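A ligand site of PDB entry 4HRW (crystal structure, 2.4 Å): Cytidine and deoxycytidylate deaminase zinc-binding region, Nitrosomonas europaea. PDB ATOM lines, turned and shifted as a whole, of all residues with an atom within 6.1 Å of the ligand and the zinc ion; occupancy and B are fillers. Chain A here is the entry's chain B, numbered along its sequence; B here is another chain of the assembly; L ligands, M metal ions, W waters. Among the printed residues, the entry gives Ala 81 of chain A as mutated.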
ATOM      1  N   PHE A  50     -13.162 -24.195  19.972  1.00  0.00           N
ATOM      2  CA  PHE A  50     -14.333 -23.341  19.786  1.00  0.00           C
ATOM      3  C   PHE A  50     -14.557 -22.452  21.004  1.00  0.00           C
ATOM      4  O   PHE A  50     -14.325 -22.875  22.134  1.00  0.00           O
ATOM      5  CB  PHE A  50     -15.593 -24.184  19.565  1.00  0.00           C
ATOM      6  CG  PHE A  50     -15.502 -25.125  18.398  1.00  0.00           C
ATOM      7  CD1 PHE A  50     -15.734 -24.662  17.105  1.00  0.00           C
ATOM      8  CD2 PHE A  50     -15.174 -26.455  18.582  1.00  0.00           C
ATOM      9  CE1 PHE A  50     -15.624 -25.517  16.020  1.00  0.00           C
ATOM     10  CE2 PHE A  50     -15.060 -27.325  17.486  1.00  0.00           C
ATOM     11  CZ  PHE A  50     -15.297 -26.847  16.204  1.00  0.00           C
ATOM     12  N   ALA A  51     -15.027 -21.234  20.754  1.00  0.00           N
ATOM     13  CA  ALA A  51     -15.336 -20.284  21.811  1.00  0.00           C
ATOM     14  C   ALA A  51     -16.328 -19.252  21.309  1.00  0.00           C
ATOM     15  O   ALA A  51     -16.465 -19.017  20.112  1.00  0.00           O
ATOM     16  CB  ALA A  51     -14.060 -19.587  22.299  1.00  0.00           C
ATOM     17  N   THR A  67     -16.792 -21.738  26.034  1.00  0.00           N
ATOM     18  CA  THR A  67     -15.917 -22.490  25.142  1.00  0.00           C
ATOM     19  C   THR A  67     -16.340 -23.938  25.181  1.00  0.00           C
ATOM     20  O   THR A  67     -17.033 -24.365  26.105  1.00  0.00           O
ATOM     21  CB  THR A  67     -14.418 -22.398  25.582  1.00  0.00           C
ATOM     22  OG1 THR A  67     -14.249 -23.041  26.853  1.00  0.00           O
ATOM     23  CG2 THR A  67     -13.983 -20.935  25.724  1.00  0.00           C
ATOM     24  N   ASN A  68     -15.953 -24.704  24.164  1.00  0.00           N
ATOM     25  CA  ASN A  68     -16.276 -26.115  24.142  1.00  0.00           C
ATOM     26  C   ASN A  68     -15.570 -26.750  25.333  1.00  0.00           C
ATOM     27  O   ASN A  68     -14.370 -26.565  25.511  1.00  0.00           O
ATOM     28  CB  ASN A  68     -15.779 -26.749  22.844  1.00  0.00           C
ATOM     29  CG  ASN A  68     -15.966 -28.253  22.816  1.00  0.00           C
ATOM     30  OD1 ASN A  68     -15.494 -28.973  23.703  1.00  0.00           O
ATOM     31  ND2 ASN A  68     -16.663 -28.738  21.801  1.00  0.00           N
ATOM     32  N   ARG A  69     -16.328 -27.466  26.155  1.00  0.00           N
ATOM     33  CA  ARG A  69     -15.778 -28.137  27.328  1.00  0.00           C
ATOM     34  C   ARG A  69     -16.327 -29.558  27.399  1.00  0.00           C
ATOM     35  O   ARG A  69     -16.378 -30.169  28.455  1.00  0.00           O
ATOM     36  CB  ARG A  69     -16.150 -27.374  28.607  1.00  0.00           C
ATOM     37  CG  ARG A  69     -15.676 -25.923  28.639  1.00  0.00           C
ATOM     38  CD  ARG A  69     -14.164 -25.808  28.445  1.00  0.00           C
ATOM     39  NE  ARG A  69     -13.435 -26.512  29.494  1.00  0.00           N
ATOM     40  CZ  ARG A  69     -12.122 -26.677  29.501  1.00  0.00           C
ATOM     41  NH1 ARG A  69     -11.370 -26.179  28.521  1.00  0.00           N
ATOM     42  NH2 ARG A  69     -11.542 -27.313  30.515  1.00  0.00           N
ATOM     43  N   VAL A  70     -16.724 -30.072  26.236  1.00  0.00           N
ATOM     44  CA  VAL A  70     -17.291 -31.406  26.103  1.00  0.00           C
ATOM     45  C   VAL A  70     -16.519 -32.535  26.807  1.00  0.00           C
ATOM     46  O   VAL A  70     -17.017 -33.128  27.766  1.00  0.00           O
ATOM     47  CB  VAL A  70     -17.461 -31.763  24.620  1.00  0.00           C
ATOM     48  CG1 VAL A  70     -17.965 -33.211  24.480  1.00  0.00           C
ATOM     49  CG2 VAL A  70     -18.439 -30.777  23.955  1.00  0.00           C
ATOM     50  N   SER A  76     -21.834 -33.480  26.373  1.00  0.00           N
ATOM     51  CA  SER A  76     -21.936 -33.247  24.944  1.00  0.00           C
ATOM     52  C   SER A  76     -22.675 -31.965  24.593  1.00  0.00           C
ATOM     53  O   SER A  76     -22.637 -31.526  23.434  1.00  0.00           O
ATOM     54  CB  SER A  76     -22.591 -34.455  24.256  1.00  0.00           C
ATOM     55  OG  SER A  76     -23.782 -34.857  24.926  1.00  0.00           O
ATOM     56  N   ALA A  78     -21.985 -29.155  26.123  1.00  0.00           N
ATOM     57  CA  ALA A  78     -21.072 -28.086  26.479  1.00  0.00           C
ATOM     58  C   ALA A  78     -20.343 -27.415  25.315  1.00  0.00           C
ATOM     59  O   ALA A  78     -19.125 -27.292  25.320  1.00  0.00           O
ATOM     60  CB  ALA A  78     -20.044 -28.612  27.497  1.00  0.00           C
ATOM     61  N   HIS A  79     -21.090 -26.971  24.303  1.00  0.00           N
ATOM     62  CA  HIS A  79     -20.479 -26.285  23.173  1.00  0.00           C
ATOM     63  C   HIS A  79     -20.284 -24.810  23.532  1.00  0.00           C
ATOM     64  O   HIS A  79     -20.975 -24.282  24.412  1.00  0.00           O
ATOM     65  CB  HIS A  79     -21.340 -26.418  21.910  1.00  0.00           C
ATOM     66  CG  HIS A  79     -21.348 -27.814  21.360  1.00  0.00           C
ATOM     67  ND1 HIS A  79     -21.945 -28.133  20.155  1.00  0.00           N
ATOM     68  CD2 HIS A  79     -20.841 -28.967  21.839  1.00  0.00           C
ATOM     69  CE1 HIS A  79     -21.793 -29.428  19.927  1.00  0.00           C
ATOM     70  NE2 HIS A  79     -21.121 -29.956  20.933  1.00  0.00           N
ATOM     71  N   ALA A  80     -19.343 -24.160  22.867  1.00  0.00           N
ATOM     72  CA  ALA A  80     -19.056 -22.752  23.145  1.00  0.00           C
ATOM     73  C   ALA A  80     -20.292 -21.875  23.274  1.00  0.00           C
ATOM     74  O   ALA A  80     -20.414 -21.118  24.240  1.00  0.00           O
ATOM     75  CB  ALA A  80     -18.132 -22.195  22.067  1.00  0.00           C
ATOM     76  N   ALA A  81     -21.209 -21.981  22.322  1.00  0.00           N
ATOM     77  CA  ALA A  81     -22.418 -21.170  22.322  1.00  0.00           C
ATOM     78  C   ALA A  81     -23.355 -21.443  23.511  1.00  0.00           C
ATOM     79  O   ALA A  81     -23.886 -20.514  24.108  1.00  0.00           O
ATOM     80  CB  ALA A  81     -23.169 -21.331  20.985  1.00  0.00           C
ATOM     81  N   ILE A  82     -23.563 -22.717  23.846  1.00  0.00           N
ATOM     82  CA  ILE A  82     -24.439 -23.058  24.961  1.00  0.00           C
ATOM     83  C   ILE A  82     -24.028 -22.390  26.270  1.00  0.00           C
ATOM     84  O   ILE A  82     -24.840 -21.732  26.931  1.00  0.00           O
ATOM     85  CB  ILE A  82     -24.475 -24.576  25.215  1.00  0.00           C
ATOM     86  CG1 ILE A  82     -25.162 -25.287  24.042  1.00  0.00           C
ATOM     87  CG2 ILE A  82     -25.237 -24.870  26.512  1.00  0.00           C
ATOM     88  CD1 ILE A  82     -26.621 -24.930  23.877  1.00  0.00           C
ATOM     89  N   ALA A 111     -17.058 -20.210  15.228  1.00  0.00           N
ATOM     90  CA  ALA A 111     -17.477 -21.054  14.109  1.00  0.00           C
ATOM     91  C   ALA A 111     -18.997 -21.047  14.019  1.00  0.00           C
ATOM     92  O   ALA A 111     -19.679 -20.757  15.007  1.00  0.00           O
ATOM     93  CB  ALA A 111     -16.966 -22.485  14.303  1.00  0.00           C
ATOM     94  N   GLU A 112     -19.529 -21.361  12.836  1.00  0.00           N
ATOM     95  CA  GLU A 112     -20.977 -21.380  12.672  1.00  0.00           C
ATOM     96  C   GLU A 112     -21.551 -22.489  13.541  1.00  0.00           C
ATOM     97  O   GLU A 112     -21.030 -23.602  13.574  1.00  0.00           O
ATOM     98  CB  GLU A 112     -21.348 -21.593  11.199  1.00  0.00           C
ATOM     99  CG  GLU A 112     -20.733 -20.558  10.292  1.00  0.00           C
ATOM    100  CD  GLU A 112     -21.155 -20.688   8.843  1.00  0.00           C
ATOM    101  OE1 GLU A 112     -21.275 -21.831   8.352  1.00  0.00           O
ATOM    102  OE2 GLU A 112     -21.356 -19.648   8.195  1.00  0.00           O
ATOM    103  N   PRO A 113     -22.641 -22.197  14.256  1.00  0.00           N
ATOM    104  CA  PRO A 113     -23.302 -23.161  15.150  1.00  0.00           C
ATOM    105  C   PRO A 113     -23.807 -24.442  14.522  1.00  0.00           C
ATOM    106  O   PRO A 113     -24.181 -24.475  13.349  1.00  0.00           O
ATOM    107  CB  PRO A 113     -24.433 -22.330  15.746  1.00  0.00           C
ATOM    108  CG  PRO A 113     -24.815 -21.443  14.609  1.00  0.00           C
ATOM    109  CD  PRO A 113     -23.463 -20.986  14.093  1.00  0.00           C
ATOM    110  N   CYS A 114     -23.829 -25.504  15.319  1.00  0.00           N
ATOM    111  CA  CYS A 114     -24.310 -26.802  14.887  1.00  0.00           C
ATOM    112  C   CYS A 114     -25.818 -26.778  15.083  1.00  0.00           C
ATOM    113  O   CYS A 114     -26.361 -25.817  15.664  1.00  0.00           O
ATOM    114  CB  CYS A 114     -23.695 -27.933  15.721  1.00  0.00           C
ATOM    115  SG  CYS A 114     -24.244 -28.010  17.466  1.00  0.00           S
ATOM    116  N   VAL A 115     -26.512 -27.809  14.626  1.00  0.00           N
ATOM    117  CA  VAL A 115     -27.959 -27.841  14.767  1.00  0.00           C
ATOM    118  C   VAL A 115     -28.390 -27.565  16.206  1.00  0.00           C
ATOM    119  O   VAL A 115     -29.373 -26.847  16.438  1.00  0.00           O
ATOM    120  CB  VAL A 115     -28.541 -29.203  14.292  1.00  0.00           C
ATOM    121  CG1 VAL A 115     -27.980 -30.342  15.132  1.00  0.00           C
ATOM    122  CG2 VAL A 115     -30.063 -29.161  14.349  1.00  0.00           C
ATOM    123  N   MET A 116     -27.654 -28.099  17.180  1.00  0.00           N
ATOM    124  CA  MET A 116     -28.000 -27.869  18.579  1.00  0.00           C
ATOM    125  C   MET A 116     -27.889 -26.401  18.965  1.00  0.00           C
ATOM    126  O   MET A 116     -28.852 -25.784  19.419  1.00  0.00           O
ATOM    127  CB  MET A 116     -27.117 -28.707  19.510  1.00  0.00           C
ATOM    128  CG  MET A 116     -27.372 -28.439  20.985  1.00  0.00           C
ATOM    129  SD  MET A 116     -26.423 -29.472  22.114  1.00  0.00           S
ATOM    130  CE  MET A 116     -24.775 -28.676  22.000  1.00  0.00           C
ATOM    131  N   CYS A 117     -26.687 -25.835  18.799  1.00  0.00           N
ATOM    132  CA  CYS A 117     -26.463 -24.431  19.130  1.00  0.00           C
ATOM    133  C   CYS A 117     -27.383 -23.537  18.316  1.00  0.00           C
ATOM    134  O   CYS A 117     -27.768 -22.455  18.761  1.00  0.00           O
ATOM    135  CB  CYS A 117     -25.007 -24.049  18.873  1.00  0.00           C
ATOM    136  SG  CYS A 117     -23.897 -24.748  20.100  1.00  0.00           S
ATOM    137  N   PHE A 118     -27.729 -23.989  17.123  1.00  0.00           N
ATOM    138  CA  PHE A 118     -28.625 -23.255  16.226  1.00  0.00           C
ATOM    139  C   PHE A 118     -29.884 -22.944  17.037  1.00  0.00           C
ATOM    140  O   PHE A 118     -30.320 -21.794  17.095  1.00  0.00           O
ATOM    141  CB  PHE A 118     -28.964 -24.132  15.012  1.00  0.00           C
ATOM    142  CG  PHE A 118     -30.060 -23.598  14.148  1.00  0.00           C
ATOM    143  CD1 PHE A 118     -29.945 -22.371  13.500  1.00  0.00           C
ATOM    144  CD2 PHE A 118     -31.232 -24.333  13.975  1.00  0.00           C
ATOM    145  CE1 PHE A 118     -30.957 -21.884  12.687  1.00  0.00           C
ATOM    146  CE2 PHE A 118     -32.266 -23.852  13.160  1.00  0.00           C
ATOM    147  CZ  PHE A 118     -32.121 -22.631  12.516  1.00  0.00           C
ATOM    148  N   VAL A 138     -15.312 -26.112   9.778  1.00  0.00           N
ATOM    149  CA  VAL A 138     -15.477 -26.942  10.969  1.00  0.00           C
ATOM    150  C   VAL A 138     -15.484 -28.414  10.563  1.00  0.00           C
ATOM    151  O   VAL A 138     -14.783 -29.244  11.152  1.00  0.00           O
ATOM    152  CB  VAL A 138     -16.803 -26.598  11.685  1.00  0.00           C
ATOM    153  CG1 VAL A 138     -16.973 -27.474  12.921  1.00  0.00           C
ATOM    154  CG2 VAL A 138     -16.829 -25.141  12.079  1.00  0.00           C
ATOM    155  N   PHE A 143     -15.200 -31.979  12.782  1.00  0.00           N
ATOM    156  CA  PHE A 143     -16.337 -31.610  13.619  1.00  0.00           C
ATOM    157  C   PHE A 143     -17.658 -31.500  12.862  1.00  0.00           C
ATOM    158  O   PHE A 143     -17.795 -30.729  11.908  1.00  0.00           O
ATOM    159  CB  PHE A 143     -16.041 -30.307  14.372  1.00  0.00           C
ATOM    160  CG  PHE A 143     -15.138 -30.509  15.557  1.00  0.00           C
ATOM    161  CD1 PHE A 143     -15.638 -31.065  16.731  1.00  0.00           C
ATOM    162  CD2 PHE A 143     -13.788 -30.178  15.487  1.00  0.00           C
ATOM    163  CE1 PHE A 143     -14.804 -31.295  17.817  1.00  0.00           C
ATOM    164  CE2 PHE A 143     -12.943 -30.412  16.565  1.00  0.00           C
ATOM    165  CZ  PHE A 143     -13.452 -30.972  17.742  1.00  0.00           C
ATOM    166  N   ASP A 144     -18.618 -32.303  13.308  1.00  0.00           N
ATOM    167  CA  ASP A 144     -19.948 -32.396  12.728  1.00  0.00           C
ATOM    168  C   ASP A 144     -20.862 -31.234  13.149  1.00  0.00           C
ATOM    169  O   ASP A 144     -20.820 -30.775  14.287  1.00  0.00           O
ATOM    170  CB  ASP A 144     -20.584 -33.712  13.184  1.00  0.00           C
ATOM    171  CG  ASP A 144     -21.591 -34.274  12.194  1.00  0.00           C
ATOM    172  OD1 ASP A 144     -22.369 -33.487  11.596  1.00  0.00           O
ATOM    173  OD2 ASP A 144     -21.609 -35.505  12.033  1.00  0.00           O
ATOM    174  N   GLU A 145     -21.700 -30.766  12.224  1.00  0.00           N
ATOM    175  CA  GLU A 145     -22.625 -29.668  12.516  1.00  0.00           C
ATOM    176  C   GLU A 145     -24.053 -30.226  12.641  1.00  0.00           C
ATOM    177  O   GLU A 145     -25.005 -29.504  12.933  1.00  0.00           O
ATOM    178  CB  GLU A 145     -22.573 -28.606  11.412  1.00  0.00           C
ATOM    179  CG  GLU A 145     -21.204 -27.933  11.241  1.00  0.00           C
ATOM    180  CD  GLU A 145     -20.981 -26.736  12.185  1.00  0.00           C
ATOM    181  OE1 GLU A 145     -20.939 -26.905  13.425  1.00  0.00           O
ATOM    182  OE2 GLU A 145     -20.851 -25.596  11.666  1.00  0.00           O
ATOM    183  N   TRP B 123     -26.027 -35.677  19.518  1.00  0.00           N
ATOM    184  CA  TRP B 123     -24.689 -35.595  20.100  1.00  0.00           C
ATOM    185  C   TRP B 123     -24.554 -36.380  21.413  1.00  0.00           C
ATOM    186  O   TRP B 123     -23.442 -36.714  21.821  1.00  0.00           O
ATOM    187  CB  TRP B 123     -24.319 -34.131  20.390  1.00  0.00           C
ATOM    188  CG  TRP B 123     -24.349 -33.197  19.198  1.00  0.00           C
ATOM    189  CD1 TRP B 123     -24.636 -31.863  19.223  1.00  0.00           C
ATOM    190  CD2 TRP B 123     -24.059 -33.517  17.831  1.00  0.00           C
ATOM    191  NE1 TRP B 123     -24.547 -31.325  17.963  1.00  0.00           N
ATOM    192  CE2 TRP B 123     -24.187 -32.328  17.092  1.00  0.00           C
ATOM    193  CE3 TRP B 123     -23.699 -34.696  17.172  1.00  0.00           C
ATOM    194  CZ2 TRP B 123     -23.985 -32.274  15.710  1.00  0.00           C
ATOM    195  CZ3 TRP B 123     -23.493 -34.646  15.798  1.00  0.00           C
ATOM    196  CH2 TRP B 123     -23.631 -33.441  15.086  1.00  0.00           C
HETATM  197  C1  LIG L   1     -18.844 -26.621  18.613  1.00  0.00           C
HETATM  198  N1  LIG L   1     -19.217 -26.959  17.300  1.00  0.00           N
HETATM  199  C2  LIG L   1     -19.175 -28.275  16.874  1.00  0.00           C
HETATM  200  N2  LIG L   1     -19.530 -28.613  15.641  1.00  0.00           N
HETATM  201  N3  LIG L   1     -18.752 -29.271  17.826  1.00  0.00           N
HETATM  202  C3  LIG L   1     -18.391 -28.860  19.156  1.00  0.00           C
HETATM  203  O1  LIG L   1     -18.032 -29.764  19.949  1.00  0.00           O
HETATM  204  C4  LIG L   1     -18.450 -27.532  19.521  1.00  0.00           C
HETATM  205  N4  LIG L   1     -18.194 -26.798  20.615  1.00  0.00           N
HETATM  206  N5  LIG L   1     -18.412 -25.644  20.388  1.00  0.00           N
HETATM  207  N6  LIG L   1     -18.777 -25.452  19.295  1.00  0.00           N
HETATM  208 ZN    ZN M   1     -22.867 -26.605  18.891  1.00  0.00          ZN
HETATM  209  O   HOH W   1     -20.372 -31.824  17.381  1.00  0.00           O
HETATM  210  O   HOH W   2     -19.211 -24.392  15.352  1.00  0.00           O
HETATM  211  O   HOH W   3     -20.993 -23.202  19.604  1.00  0.00           O
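The backbone carbonyl oxygen of Ser 76 is in hydrogen-bond range of a ring nitrogen (NE2) of His 79, at 3.3 Å. The side-chain sulfur (SG) of Cys 114 sits close to the backbone NH (N) of Met 116. NE1 of Trp 123 of chain B sits close to SG of Cys 114. N of Asn 68 is in hydrogen-bond range of O of Phe 50 (3.2 Å). The side-chain amide oxygen (OD1) of Asn 68 lies within hydrogen-bond range of the backbone NH (N) of Val 70. The backbone NH (N) of Val 115 is in hydrogen-bond range of the backbone carbonyl oxygen (O) of Glu 145 (2.8 Å). The backbone NH (N) of Phe 143 lies within hydrogen-bond range of the backbone carbonyl oxygen (O) of Val 138.
The zinc ion is bound by a ring nitrogen (ND1) of His 79 (2.2 Å), the side-chain sulfur (SG) of Cys 114 (2.4 Å) and the side-chain sulfur (SG) of Cys 117 (2.4 Å).
Of the 25 residues printed, 3 come within 4 Å of the zinc ion. The nearest printed residue that does not touch the zinc ion is Met 116 (4.2 Å).
CB of Phe 50 touches N5 of the ligand (3.3 Å). Val 138 touches the ligand. CD1 of Phe 143 touches N3 of the ligand, 3.8 Å away. Hydrophobic or aromatic side chains within 4 Å of the ligand: Phe 50, His 79, Ala 80, Val 138 and Phe 143. Within 4 Å of the ligand: Phe 50, Asn 68, His 79, Ala 80, Val 138, Phe 143, Asp 144 and Glu 145.
A ring nitrogen (NE2) of His 79 is in hydrogen-bond range of an oxygen (O1) of the ligand (3.2 Å). ND2 of Asn 68 lies within hydrogen-bond range of O1 of the ligand. The backbone carbonyl oxygen (O) of Asp 144 lies within hydrogen-bond range of a nitrogen (N2) of the ligand (2.9 Å). The backbone NH of Ala 80 lies within hydrogen-bond range of a nitrogen (N5) of the ligand (3.0 Å). The side-chain carboxylate of Glu 145 sits at hydrogen-bond distance from a nitrogen (N2) of the ligand (3.1 Å).
Water W1 lies within hydrogen-bond range of N3 of the ligand (3.1 Å) and O of Asp 144 (3.3 Å). Water W3 lies within hydrogen-bond range of the backbone NH (N) of Ala 81 (3.0 Å) and a nitrogen (N6) of the ligand (3.2 Å). Water W2 lies within hydrogen-bond range of O of Glu 112 (2.7 Å) and N1 of the ligand (3.2 Å).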
